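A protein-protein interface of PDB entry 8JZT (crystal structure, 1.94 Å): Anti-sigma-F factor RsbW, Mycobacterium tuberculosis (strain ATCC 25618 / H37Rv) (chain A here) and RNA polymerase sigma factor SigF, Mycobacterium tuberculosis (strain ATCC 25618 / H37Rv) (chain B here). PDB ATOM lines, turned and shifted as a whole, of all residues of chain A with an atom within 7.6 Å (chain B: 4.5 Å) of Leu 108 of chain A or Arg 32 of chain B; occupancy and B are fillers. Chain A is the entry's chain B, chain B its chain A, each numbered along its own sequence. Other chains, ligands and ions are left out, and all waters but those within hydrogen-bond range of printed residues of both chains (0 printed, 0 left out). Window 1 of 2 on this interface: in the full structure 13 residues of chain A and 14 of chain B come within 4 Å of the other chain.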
ATOM      1  N   ASP A  44      26.376 -12.424 -10.456  1.00  0.00           N
ATOM      2  CA  ASP A  44      25.820 -12.979  -9.228  1.00  0.00           C
ATOM      3  C   ASP A  44      26.900 -13.088  -8.153  1.00  0.00           C
ATOM      4  O   ASP A  44      26.646 -12.832  -6.966  1.00  0.00           O
ATOM      5  CB  ASP A  44      25.178 -14.329  -9.516  1.00  0.00           C
ATOM      6  CG  ASP A  44      23.870 -14.198 -10.278  1.00  0.00           C
ATOM      7  OD1 ASP A  44      23.021 -13.395  -9.856  1.00  0.00           O
ATOM      8  OD2 ASP A  44      23.672 -14.910 -11.288  1.00  0.00           O
ATOM      9  N   ALA A  45      28.126 -13.426  -8.560  1.00  0.00           N
ATOM     10  CA  ALA A  45      29.228 -13.487  -7.606  1.00  0.00           C
ATOM     11  C   ALA A  45      29.566 -12.104  -7.064  1.00  0.00           C
ATOM     12  O   ALA A  45      29.912 -11.961  -5.881  1.00  0.00           O
ATOM     13  CB  ALA A  45      30.449 -14.129  -8.262  1.00  0.00           C
ATOM     14  N   VAL A  46      29.462 -11.070  -7.901  1.00  0.00           N
ATOM     15  CA  VAL A  46      29.773  -9.714  -7.437  1.00  0.00           C
ATOM     16  C   VAL A  46      28.745  -9.249  -6.410  1.00  0.00           C
ATOM     17  O   VAL A  46      29.094  -8.668  -5.378  1.00  0.00           O
ATOM     18  CB  VAL A  46      29.841  -8.731  -8.624  1.00  0.00           C
ATOM     19  CG1 VAL A  46      29.947  -7.290  -8.118  1.00  0.00           C
ATOM     20  CG2 VAL A  46      30.992  -9.074  -9.588  1.00  0.00           C
ATOM     21  N   ALA A  47      27.454  -9.446  -6.718  1.00  0.00           N
ATOM     22  CA  ALA A  47      26.377  -9.059  -5.808  1.00  0.00           C
ATOM     23  C   ALA A  47      26.481  -9.774  -4.456  1.00  0.00           C
ATOM     24  O   ALA A  47      26.283  -9.153  -3.403  1.00  0.00           O
ATOM     25  CB  ALA A  47      25.024  -9.355  -6.460  1.00  0.00           C
ATOM     26  N   ASP A  48      26.761 -11.084  -4.458  1.00  0.00           N
ATOM     27  CA  ASP A  48      26.997 -11.782  -3.189  1.00  0.00           C
ATOM     28  C   ASP A  48      28.205 -11.204  -2.466  1.00  0.00           C
ATOM     29  O   ASP A  48      28.159 -10.948  -1.257  1.00  0.00           O
ATOM     30  CB  ASP A  48      27.228 -13.267  -3.427  1.00  0.00           C
ATOM     31  CG  ASP A  48      25.957 -14.033  -3.697  1.00  0.00           C
ATOM     32  OD1 ASP A  48      24.838 -13.544  -3.414  1.00  0.00           O
ATOM     33  OD2 ASP A  48      26.106 -15.172  -4.172  1.00  0.00           O
ATOM     34  N   LEU A  49      29.312 -11.004  -3.187  1.00  0.00           N
ATOM     35  CA  LEU A  49      30.514 -10.482  -2.535  1.00  0.00           C
ATOM     36  C   LEU A  49      30.270  -9.109  -1.911  1.00  0.00           C
ATOM     37  O   LEU A  49      30.789  -8.805  -0.830  1.00  0.00           O
ATOM     38  CB  LEU A  49      31.663 -10.418  -3.543  1.00  0.00           C
ATOM     39  CG  LEU A  49      32.993  -9.958  -2.936  1.00  0.00           C
ATOM     40  CD1 LEU A  49      33.476 -10.932  -1.859  1.00  0.00           C
ATOM     41  CD2 LEU A  49      34.036  -9.787  -4.055  1.00  0.00           C
ATOM     42  N   ARG A  50      29.503  -8.263  -2.581  1.00  0.00           N
ATOM     43  CA  ARG A  50      29.219  -6.922  -2.024  1.00  0.00           C
ATOM     44  C   ARG A  50      28.496  -7.066  -0.674  1.00  0.00           C
ATOM     45  O   ARG A  50      28.871  -6.366   0.269  1.00  0.00           O
ATOM     46  CB  ARG A  50      28.443  -6.093  -3.048  1.00  0.00           C
ATOM     47  CG  ARG A  50      29.328  -5.633  -4.194  1.00  0.00           C
ATOM     48  CD  ARG A  50      28.707  -4.469  -4.931  1.00  0.00           C
ATOM     49  NE  ARG A  50      27.411  -4.100  -4.354  1.00  0.00           N
ATOM     50  CZ  ARG A  50      26.900  -2.881  -4.377  1.00  0.00           C
ATOM     51  NH1 ARG A  50      26.888  -2.190  -5.502  1.00  0.00           N
ATOM     52  NH2 ARG A  50      26.408  -2.358  -3.268  1.00  0.00           N
ATOM     53  N   LEU A  51      27.498  -7.946  -0.604  1.00  0.00           N
ATOM     54  CA  LEU A  51      26.811  -8.169   0.670  1.00  0.00           C
ATOM     55  C   LEU A  51      27.766  -8.707   1.733  1.00  0.00           C
ATOM     56  O   LEU A  51      27.681  -8.328   2.910  1.00  0.00           O
ATOM     57  CB  LEU A  51      25.660  -9.164   0.479  1.00  0.00           C
ATOM     58  CG  LEU A  51      24.438  -8.753  -0.320  1.00  0.00           C
ATOM     59  CD1 LEU A  51      23.507  -9.971  -0.460  1.00  0.00           C
ATOM     60  CD2 LEU A  51      23.733  -7.600   0.380  1.00  0.00           C
ATOM     61  N   ALA A  52      28.632  -9.643   1.360  1.00  0.00           N
ATOM     62  CA  ALA A  52      29.538 -10.211   2.356  1.00  0.00           C
ATOM     63  C   ALA A  52      30.536  -9.169   2.850  1.00  0.00           C
ATOM     64  O   ALA A  52      30.889  -9.151   4.036  1.00  0.00           O
ATOM     65  CB  ALA A  52      30.260 -11.430   1.775  1.00  0.00           C
ATOM     66  N   VAL A  53      31.037  -8.316   1.956  1.00  0.00           N
ATOM     67  CA  VAL A  53      32.002  -7.311   2.392  1.00  0.00           C
ATOM     68  C   VAL A  53      31.344  -6.313   3.329  1.00  0.00           C
ATOM     69  O   VAL A  53      31.960  -5.858   4.308  1.00  0.00           O
ATOM     70  CB  VAL A  53      32.650  -6.604   1.189  1.00  0.00           C
ATOM     71  CG1 VAL A  53      33.524  -5.443   1.686  1.00  0.00           C
ATOM     72  CG2 VAL A  53      33.475  -7.614   0.367  1.00  0.00           C
ATOM     73  N   GLU A  55      28.881  -7.047   5.346  1.00  0.00           N
ATOM     74  CA  GLU A  55      28.747  -7.744   6.632  1.00  0.00           C
ATOM     75  C   GLU A  55      30.069  -7.722   7.400  1.00  0.00           C
ATOM     76  O   GLU A  55      30.109  -7.407   8.590  1.00  0.00           O
ATOM     77  CB  GLU A  55      28.281  -9.181   6.402  1.00  0.00           C
ATOM     78  CG  GLU A  55      28.293 -10.069   7.660  1.00  0.00           C
ATOM     79  CD  GLU A  55      27.131  -9.764   8.600  1.00  0.00           C
ATOM     80  OE1 GLU A  55      26.203  -9.038   8.175  1.00  0.00           O
ATOM     81  OE2 GLU A  55      27.131 -10.271   9.742  1.00  0.00           O
ATOM     82  N   SER A 101      26.348 -14.639  11.515  1.00  0.00           N
ATOM     83  CA  SER A 101      27.293 -13.938  10.654  1.00  0.00           C
ATOM     84  C   SER A 101      28.215 -14.899   9.907  1.00  0.00           C
ATOM     85  O   SER A 101      28.411 -14.772   8.693  1.00  0.00           O
ATOM     86  CB  SER A 101      28.108 -12.961  11.495  1.00  0.00           C
ATOM     87  OG  SER A 101      29.003 -12.244  10.682  1.00  0.00           O
ATOM     88  N   TRP A 102      28.811 -15.859  10.622  1.00  0.00           N
ATOM     89  CA  TRP A 102      29.711 -16.810   9.971  1.00  0.00           C
ATOM     90  C   TRP A 102      28.995 -17.603   8.885  1.00  0.00           C
ATOM     91  O   TRP A 102      29.548 -17.831   7.799  1.00  0.00           O
ATOM     92  CB  TRP A 102      30.306 -17.777  10.999  1.00  0.00           C
ATOM     93  CG  TRP A 102      31.288 -18.730  10.383  1.00  0.00           C
ATOM     94  CD1 TRP A 102      31.098 -20.053  10.111  1.00  0.00           C
ATOM     95  CD2 TRP A 102      32.616 -18.416   9.963  1.00  0.00           C
ATOM     96  NE1 TRP A 102      32.232 -20.584   9.538  1.00  0.00           N
ATOM     97  CE2 TRP A 102      33.183 -19.605   9.451  1.00  0.00           C
ATOM     98  CE3 TRP A 102      33.386 -17.244   9.976  1.00  0.00           C
ATOM     99  CZ2 TRP A 102      34.470 -19.652   8.936  1.00  0.00           C
ATOM    100  CZ3 TRP A 102      34.662 -17.297   9.475  1.00  0.00           C
ATOM    101  CH2 TRP A 102      35.198 -18.506   8.972  1.00  0.00           C
ATOM    102  N   HIS A 103      27.764 -18.036   9.158  1.00  0.00           N
ATOM    103  CA  HIS A 103      27.030 -18.804   8.166  1.00  0.00           C
ATOM    104  C   HIS A 103      26.696 -17.945   6.954  1.00  0.00           C
ATOM    105  O   HIS A 103      26.697 -18.434   5.817  1.00  0.00           O
ATOM    106  CB  HIS A 103      25.759 -19.382   8.787  1.00  0.00           C
ATOM    107  CG  HIS A 103      26.023 -20.506   9.743  1.00  0.00           C
ATOM    108  ND1 HIS A 103      26.690 -21.660   9.377  1.00  0.00           N
ATOM    109  CD2 HIS A 103      25.681 -20.669  11.044  1.00  0.00           C
ATOM    110  CE1 HIS A 103      26.774 -22.468  10.420  1.00  0.00           C
ATOM    111  NE2 HIS A 103      26.163 -21.894  11.442  1.00  0.00           N
ATOM    112  N   VAL A 104      26.413 -16.663   7.175  1.00  0.00           N
ATOM    113  CA  VAL A 104      26.106 -15.773   6.058  1.00  0.00           C
ATOM    114  C   VAL A 104      27.324 -15.637   5.160  1.00  0.00           C
ATOM    115  O   VAL A 104      27.239 -15.753   3.930  1.00  0.00           O
ATOM    116  CB  VAL A 104      25.625 -14.403   6.577  1.00  0.00           C
ATOM    117  CG1 VAL A 104      25.737 -13.315   5.492  1.00  0.00           C
ATOM    118  CG2 VAL A 104      24.177 -14.495   7.062  1.00  0.00           C
ATOM    119  N   LEU A 105      28.481 -15.408   5.772  1.00  0.00           N
ATOM    120  CA  LEU A 105      29.705 -15.216   5.000  1.00  0.00           C
ATOM    121  C   LEU A 105      30.070 -16.473   4.232  1.00  0.00           C
ATOM    122  O   LEU A 105      30.472 -16.392   3.067  1.00  0.00           O
ATOM    123  CB  LEU A 105      30.852 -14.824   5.927  1.00  0.00           C
ATOM    124  CG  LEU A 105      30.755 -13.469   6.616  1.00  0.00           C
ATOM    125  CD1 LEU A 105      32.018 -13.249   7.504  1.00  0.00           C
ATOM    126  CD2 LEU A 105      30.587 -12.336   5.559  1.00  0.00           C
ATOM    127  N   THR A 106      29.941 -17.645   4.865  1.00  0.00           N
ATOM    128  CA  THR A 106      30.292 -18.871   4.161  1.00  0.00           C
ATOM    129  C   THR A 106      29.305 -19.185   3.040  1.00  0.00           C
ATOM    130  O   THR A 106      29.690 -19.850   2.072  1.00  0.00           O
ATOM    131  CB  THR A 106      30.420 -20.070   5.135  1.00  0.00           C
ATOM    132  OG1 THR A 106      29.265 -20.185   5.957  1.00  0.00           O
ATOM    133  CG2 THR A 106      31.593 -19.859   6.069  1.00  0.00           C
ATOM    134  N   ALA A 107      28.057 -18.699   3.117  1.00  0.00           N
ATOM    135  CA  ALA A 107      27.123 -18.894   2.009  1.00  0.00           C
ATOM    136  C   ALA A 107      27.439 -17.992   0.827  1.00  0.00           C
ATOM    137  O   ALA A 107      27.229 -18.401  -0.323  1.00  0.00           O
ATOM    138  CB  ALA A 107      25.676 -18.642   2.445  1.00  0.00           C
ATOM    139  N   LEU A 108      27.917 -16.769   1.092  1.00  0.00           N
ATOM    140  CA  LEU A 108      28.076 -15.735   0.075  1.00  0.00           C
ATOM    141  C   LEU A 108      29.436 -15.741  -0.608  1.00  0.00           C
ATOM    142  O   LEU A 108      29.554 -15.214  -1.719  1.00  0.00           O
ATOM    143  CB  LEU A 108      27.854 -14.330   0.670  1.00  0.00           C
ATOM    144  CG  LEU A 108      26.456 -14.000   1.201  1.00  0.00           C
ATOM    145  CD1 LEU A 108      26.426 -12.654   1.997  1.00  0.00           C
ATOM    146  CD2 LEU A 108      25.519 -13.941   0.027  1.00  0.00           C
ATOM    147  N   ALA A 109      30.454 -16.303   0.022  1.00  0.00           N
ATOM    148  CA  ALA A 109      31.797 -16.319  -0.537  1.00  0.00           C
ATOM    149  C   ALA A 109      32.237 -17.767  -0.692  1.00  0.00           C
ATOM    150  O   ALA A 109      31.775 -18.648   0.043  1.00  0.00           O
ATOM    151  CB  ALA A 109      32.787 -15.543   0.364  1.00  0.00           C
ATOM    152  N   ASP A 110      33.129 -18.022  -1.650  1.00  0.00           N
ATOM    153  CA  ASP A 110      33.599 -19.398  -1.826  1.00  0.00           C
ATOM    154  C   ASP A 110      34.541 -19.825  -0.713  1.00  0.00           C
ATOM    155  O   ASP A 110      34.619 -21.011  -0.385  1.00  0.00           O
ATOM    156  CB  ASP A 110      34.284 -19.561  -3.172  1.00  0.00           C
ATOM    157  CG  ASP A 110      33.324 -19.439  -4.318  1.00  0.00           C
ATOM    158  OD1 ASP A 110      32.195 -19.972  -4.209  1.00  0.00           O
ATOM    159  OD2 ASP A 110      33.679 -18.790  -5.320  1.00  0.00           O
ATOM    160  N   ASP A 111      35.269 -18.895  -0.128  1.00  0.00           N
ATOM    161  CA  ASP A 111      36.215 -19.227   0.928  1.00  0.00           C
ATOM    162  C   ASP A 111      36.180 -18.082   1.913  1.00  0.00           C
ATOM    163  O   ASP A 111      36.106 -16.928   1.494  1.00  0.00           O
ATOM    164  CB  ASP A 111      37.636 -19.442   0.373  1.00  0.00           C
ATOM    165  CG  ASP A 111      38.575 -20.102   1.375  1.00  0.00           C
ATOM    166  OD1 ASP A 111      38.144 -21.006   2.116  1.00  0.00           O
ATOM    167  OD2 ASP A 111      39.759 -19.696   1.431  1.00  0.00           O
ATOM    168  N   VAL A 112      36.167 -18.406   3.208  1.00  0.00           N
ATOM    169  CA  VAL A 112      36.206 -17.414   4.287  1.00  0.00           C
ATOM    170  C   VAL A 112      37.283 -17.848   5.275  1.00  0.00           C
ATOM    171  O   VAL A 112      37.280 -19.001   5.727  1.00  0.00           O
ATOM    172  CB  VAL A 112      34.851 -17.271   5.015  1.00  0.00           C
ATOM    173  CG1 VAL A 112      34.927 -16.148   6.053  1.00  0.00           C
ATOM    174  CG2 VAL A 112      33.742 -16.997   4.038  1.00  0.00           C
ATOM    175  N   LEU A 132      37.811 -12.888   2.315  1.00  0.00           N
ATOM    176  CA  LEU A 132      36.778 -13.525   1.517  1.00  0.00           C
ATOM    177  C   LEU A 132      37.322 -13.754   0.116  1.00  0.00           C
ATOM    178  O   LEU A 132      38.015 -12.897  -0.428  1.00  0.00           O
ATOM    179  CB  LEU A 132      35.515 -12.659   1.447  1.00  0.00           C
ATOM    180  CG  LEU A 132      34.911 -12.091   2.730  1.00  0.00           C
ATOM    181  CD1 LEU A 132      34.001 -10.921   2.393  1.00  0.00           C
ATOM    182  CD2 LEU A 132      34.143 -13.175   3.477  1.00  0.00           C
ATOM    183  N   THR A 133      37.015 -14.907  -0.465  1.00  0.00           N
ATOM    184  CA  THR A 133      37.468 -15.227  -1.811  1.00  0.00           C
ATOM    185  C   THR A 133      36.272 -15.646  -2.648  1.00  0.00           C
ATOM    186  O   THR A 133      35.471 -16.484  -2.224  1.00  0.00           O
ATOM    187  CB  THR A 133      38.519 -16.339  -1.802  1.00  0.00           C
ATOM    188  OG1 THR A 133      39.624 -15.935  -0.986  1.00  0.00           O
ATOM    189  CG2 THR A 133      39.020 -16.600  -3.211  1.00  0.00           C
ATOM    190  N   ALA A 134      36.142 -15.054  -3.821  1.00  0.00           N
ATOM    191  CA  ALA A 134      35.049 -15.370  -4.726  1.00  0.00           C
ATOM    192  C   ALA A 134      35.654 -15.757  -6.061  1.00  0.00           C
ATOM    193  O   ALA A 134      36.453 -14.997  -6.610  1.00  0.00           O
ATOM    194  CB  ALA A 134      34.100 -14.175  -4.879  1.00  0.00           C
ATOM    195  N   VAL B  28      12.802 -13.708  -0.411  1.00  0.00           N
ATOM    196  CA  VAL B  28      14.089 -13.523  -1.062  1.00  0.00           C
ATOM    197  C   VAL B  28      15.211 -14.095  -0.202  1.00  0.00           C
ATOM    198  O   VAL B  28      16.116 -14.778  -0.707  1.00  0.00           O
ATOM    199  CB  VAL B  28      14.284 -12.029  -1.381  1.00  0.00           C
ATOM    200  CG1 VAL B  28      15.717 -11.720  -1.571  1.00  0.00           C
ATOM    201  CG2 VAL B  28      13.475 -11.654  -2.620  1.00  0.00           C
ATOM    202  N   LEU B  29      15.156 -13.861   1.116  1.00  0.00           N
ATOM    203  CA  LEU B  29      16.166 -14.421   2.014  1.00  0.00           C
ATOM    204  C   LEU B  29      16.192 -15.945   1.959  1.00  0.00           C
ATOM    205  O   LEU B  29      17.270 -16.556   1.909  1.00  0.00           O
ATOM    206  CB  LEU B  29      15.917 -13.963   3.444  1.00  0.00           C
ATOM    207  CG  LEU B  29      17.162 -14.073   4.322  1.00  0.00           C
ATOM    208  CD1 LEU B  29      18.135 -12.945   4.059  1.00  0.00           C
ATOM    209  CD2 LEU B  29      16.764 -14.124   5.771  1.00  0.00           C
ATOM    210  N   VAL B  30      15.021 -16.578   1.983  1.00  0.00           N
ATOM    211  CA  VAL B  30      14.966 -18.041   2.004  1.00  0.00           C
ATOM    212  C   VAL B  30      15.430 -18.615   0.668  1.00  0.00           C
ATOM    213  O   VAL B  30      16.151 -19.622   0.621  1.00  0.00           O
ATOM    214  CB  VAL B  30      13.543 -18.502   2.370  1.00  0.00           C
ATOM    215  CG1 VAL B  30      13.373 -20.008   2.156  1.00  0.00           C
ATOM    216  CG2 VAL B  30      13.229 -18.109   3.804  1.00  0.00           C
ATOM    217  N   LEU B  31      15.042 -17.983  -0.439  1.00  0.00           N
ATOM    218  CA  LEU B  31      15.494 -18.476  -1.735  1.00  0.00           C
ATOM    219  C   LEU B  31      17.008 -18.385  -1.860  1.00  0.00           C
ATOM    220  O   LEU B  31      17.624 -19.248  -2.494  1.00  0.00           O
ATOM    221  CB  LEU B  31      14.819 -17.702  -2.870  1.00  0.00           C
ATOM    222  CG  LEU B  31      13.305 -17.868  -2.941  1.00  0.00           C
ATOM    223  CD1 LEU B  31      12.748 -16.895  -3.960  1.00  0.00           C
ATOM    224  CD2 LEU B  31      12.964 -19.300  -3.331  1.00  0.00           C
ATOM    225  N   ARG B  32      17.628 -17.363  -1.250  1.00  0.00           N
ATOM    226  CA  ARG B  32      19.087 -17.234  -1.339  1.00  0.00           C
ATOM    227  C   ARG B  32      19.797 -18.220  -0.423  1.00  0.00           C
ATOM    228  O   ARG B  32      20.728 -18.917  -0.841  1.00  0.00           O
ATOM    229  CB  ARG B  32      19.530 -15.809  -0.987  1.00  0.00           C
ATOM    230  CG  ARG B  32      21.060 -15.614  -1.021  1.00  0.00           C
ATOM    231  CD  ARG B  32      21.632 -15.993  -2.403  1.00  0.00           C
ATOM    232  NE  ARG B  32      23.094 -16.007  -2.467  1.00  0.00           N
ATOM    233  CZ  ARG B  32      23.856 -17.003  -2.040  1.00  0.00           C
ATOM    234  NH1 ARG B  32      23.338 -18.060  -1.426  1.00  0.00           N
ATOM    235  NH2 ARG B  32      25.174 -16.918  -2.191  1.00  0.00           N
ATOM    236  N   PHE B  33      19.388 -18.284   0.837  1.00  0.00           N
ATOM    237  CA  PHE B  33      20.183 -19.025   1.803  1.00  0.00           C
ATOM    238  C   PHE B  33      19.680 -20.431   2.080  1.00  0.00           C
ATOM    239  O   PHE B  33      20.446 -21.245   2.599  1.00  0.00           O
ATOM    240  CB  PHE B  33      20.286 -18.230   3.102  1.00  0.00           C
ATOM    241  CG  PHE B  33      21.072 -16.976   2.951  1.00  0.00           C
ATOM    242  CD1 PHE B  33      22.456 -17.016   2.913  1.00  0.00           C
ATOM    243  CD2 PHE B  33      20.432 -15.759   2.772  1.00  0.00           C
ATOM    244  CE1 PHE B  33      23.187 -15.863   2.746  1.00  0.00           C
ATOM    245  CE2 PHE B  33      21.164 -14.604   2.605  1.00  0.00           C
ATOM    246  CZ  PHE B  33      22.538 -14.650   2.600  1.00  0.00           C
ATOM    247  N   PHE B  34      18.439 -20.759   1.733  1.00  0.00           N
ATOM    248  CA  PHE B  34      17.981 -22.140   1.852  1.00  0.00           C
ATOM    249  C   PHE B  34      17.925 -22.875   0.529  1.00  0.00           C
ATOM    250  O   PHE B  34      18.318 -24.040   0.461  1.00  0.00           O
ATOM    251  CB  PHE B  34      16.605 -22.200   2.512  1.00  0.00           C
ATOM    252  CG  PHE B  34      16.597 -21.727   3.930  1.00  0.00           C
ATOM    253  CD1 PHE B  34      17.780 -21.394   4.573  1.00  0.00           C
ATOM    254  CD2 PHE B  34      15.404 -21.640   4.636  1.00  0.00           C
ATOM    255  CE1 PHE B  34      17.777 -20.956   5.881  1.00  0.00           C
ATOM    256  CE2 PHE B  34      15.393 -21.211   5.953  1.00  0.00           C
ATOM    257  CZ  PHE B  34      16.583 -20.870   6.576  1.00  0.00           C
ATOM    258  N   SER B  36      19.581 -21.782  -2.117  1.00  0.00           N
ATOM    259  CA  SER B  36      20.879 -21.525  -2.742  1.00  0.00           C
ATOM    260  C   SER B  36      20.738 -21.031  -4.180  1.00  0.00           C
ATOM    261  O   SER B  36      21.592 -21.302  -5.028  1.00  0.00           O
ATOM    262  CB  SER B  36      21.777 -22.763  -2.689  1.00  0.00           C
ATOM    263  OG  SER B  36      22.220 -23.004  -1.365  1.00  0.00           O
ATOM    264  N   MET B  37      19.675 -20.286  -4.465  1.00  0.00           N
ATOM    265  CA  MET B  37      19.534 -19.660  -5.768  1.00  0.00           C
ATOM    266  C   MET B  37      20.429 -18.439  -5.880  1.00  0.00           C
ATOM    267  O   MET B  37      20.723 -17.763  -4.889  1.00  0.00           O
ATOM    268  CB  MET B  37      18.072 -19.277  -6.022  1.00  0.00           C
ATOM    269  CG  MET B  37      17.147 -20.473  -5.908  1.00  0.00           C
ATOM    270  SD  MET B  37      15.392 -20.083  -6.068  1.00  0.00           S
ATOM    271  CE  MET B  37      15.331 -19.450  -7.739  1.00  0.00           C
ATOM    272  N   ILE B  42      16.709 -15.553  -8.233  1.00  0.00           N
ATOM    273  CA  ILE B  42      15.680 -15.033  -7.337  1.00  0.00           C
ATOM    274  C   ILE B  42      14.915 -13.908  -8.007  1.00  0.00           C
ATOM    275  O   ILE B  42      13.683 -13.836  -7.909  1.00  0.00           O
ATOM    276  CB  ILE B  42      16.290 -14.562  -6.008  1.00  0.00           C
ATOM    277  CG1 ILE B  42      16.843 -15.761  -5.232  1.00  0.00           C
ATOM    278  CG2 ILE B  42      15.248 -13.762  -5.212  1.00  0.00           C
ATOM    279  CD1 ILE B  42      17.925 -15.353  -4.189  1.00  0.00           C
ATOM    280  N   LEU B  57      17.918  -8.247   0.141  1.00  0.00           N
ATOM    281  CA  LEU B  57      18.851  -9.074   0.901  1.00  0.00           C
ATOM    282  C   LEU B  57      19.618  -8.228   1.911  1.00  0.00           C
ATOM    283  O   LEU B  57      19.737  -8.600   3.087  1.00  0.00           O
ATOM    284  CB  LEU B  57      19.821  -9.783  -0.045  1.00  0.00           C
ATOM    285  CG  LEU B  57      19.210 -10.990  -0.776  1.00  0.00           C
ATOM    286  CD1 LEU B  57      20.187 -11.518  -1.823  1.00  0.00           C
ATOM    287  CD2 LEU B  57      18.757 -12.104   0.221  1.00  0.00           C
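Leu 57 of chain B touches Leu 51 of chain A (CB to CD1, 3.7 Å). CD1 of Phe 33 of chain B touches CB of Ala 107 of chain A (3.6 Å). Arg 32 of chain B touches Leu 108 of chain A (NH2 to CD2, 3.7 Å).
The guanidinium group (NH2) of Arg 32 of chain B lies within salt-bridge range of the side-chain carboxylate (OD2) of Asp 48 of chain A. The backbone carbonyl oxygen (O) of Ala 107 of chain A is in hydrogen-bond range of the guanidinium group (NH2) of Arg 32 of chain B (3.1 Å).
Printed residues of chain B within 4 Å of Leu 108 of chain A: Arg 32 (3.7 Å). Arg 32 of chain B touches just these residues of chain A: Asp 48, Ala 107 and Leu 108. Printed residues of chain B within 4 Å of Leu 51 of chain A: Leu 57 (3.7 Å). Printed residues of chain A within 4 Å of Leu 57 of chain B: Leu 51. Of the printed residues of chain B, Ala 107 of chain A touches Arg 32 and Phe 33. The nearest printed residue of chain B that does not touch Leu 108 of chain A is Phe 33 of chain B (4.001 Å). The nearest residue of chain A that does not touch Arg 32 of chain B is Ala 109 of chain A (5.8 Å).
Along chain A the printed residues that touch a printed residue of chain B span positions 48 to 108. Of the 11 printed residues of chain B, 3 touch a printed residue of chain A. Printed residues of chain B that touch a printed residue of chain A: Arg 32, Phe 33 and Leu 57. Hydrophobic or aromatic side chains of chain B within 4 Å of the printed part of chain A: Phe 33 and Leu 57. Among the printed residues, 5 pairs touch across the chains.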
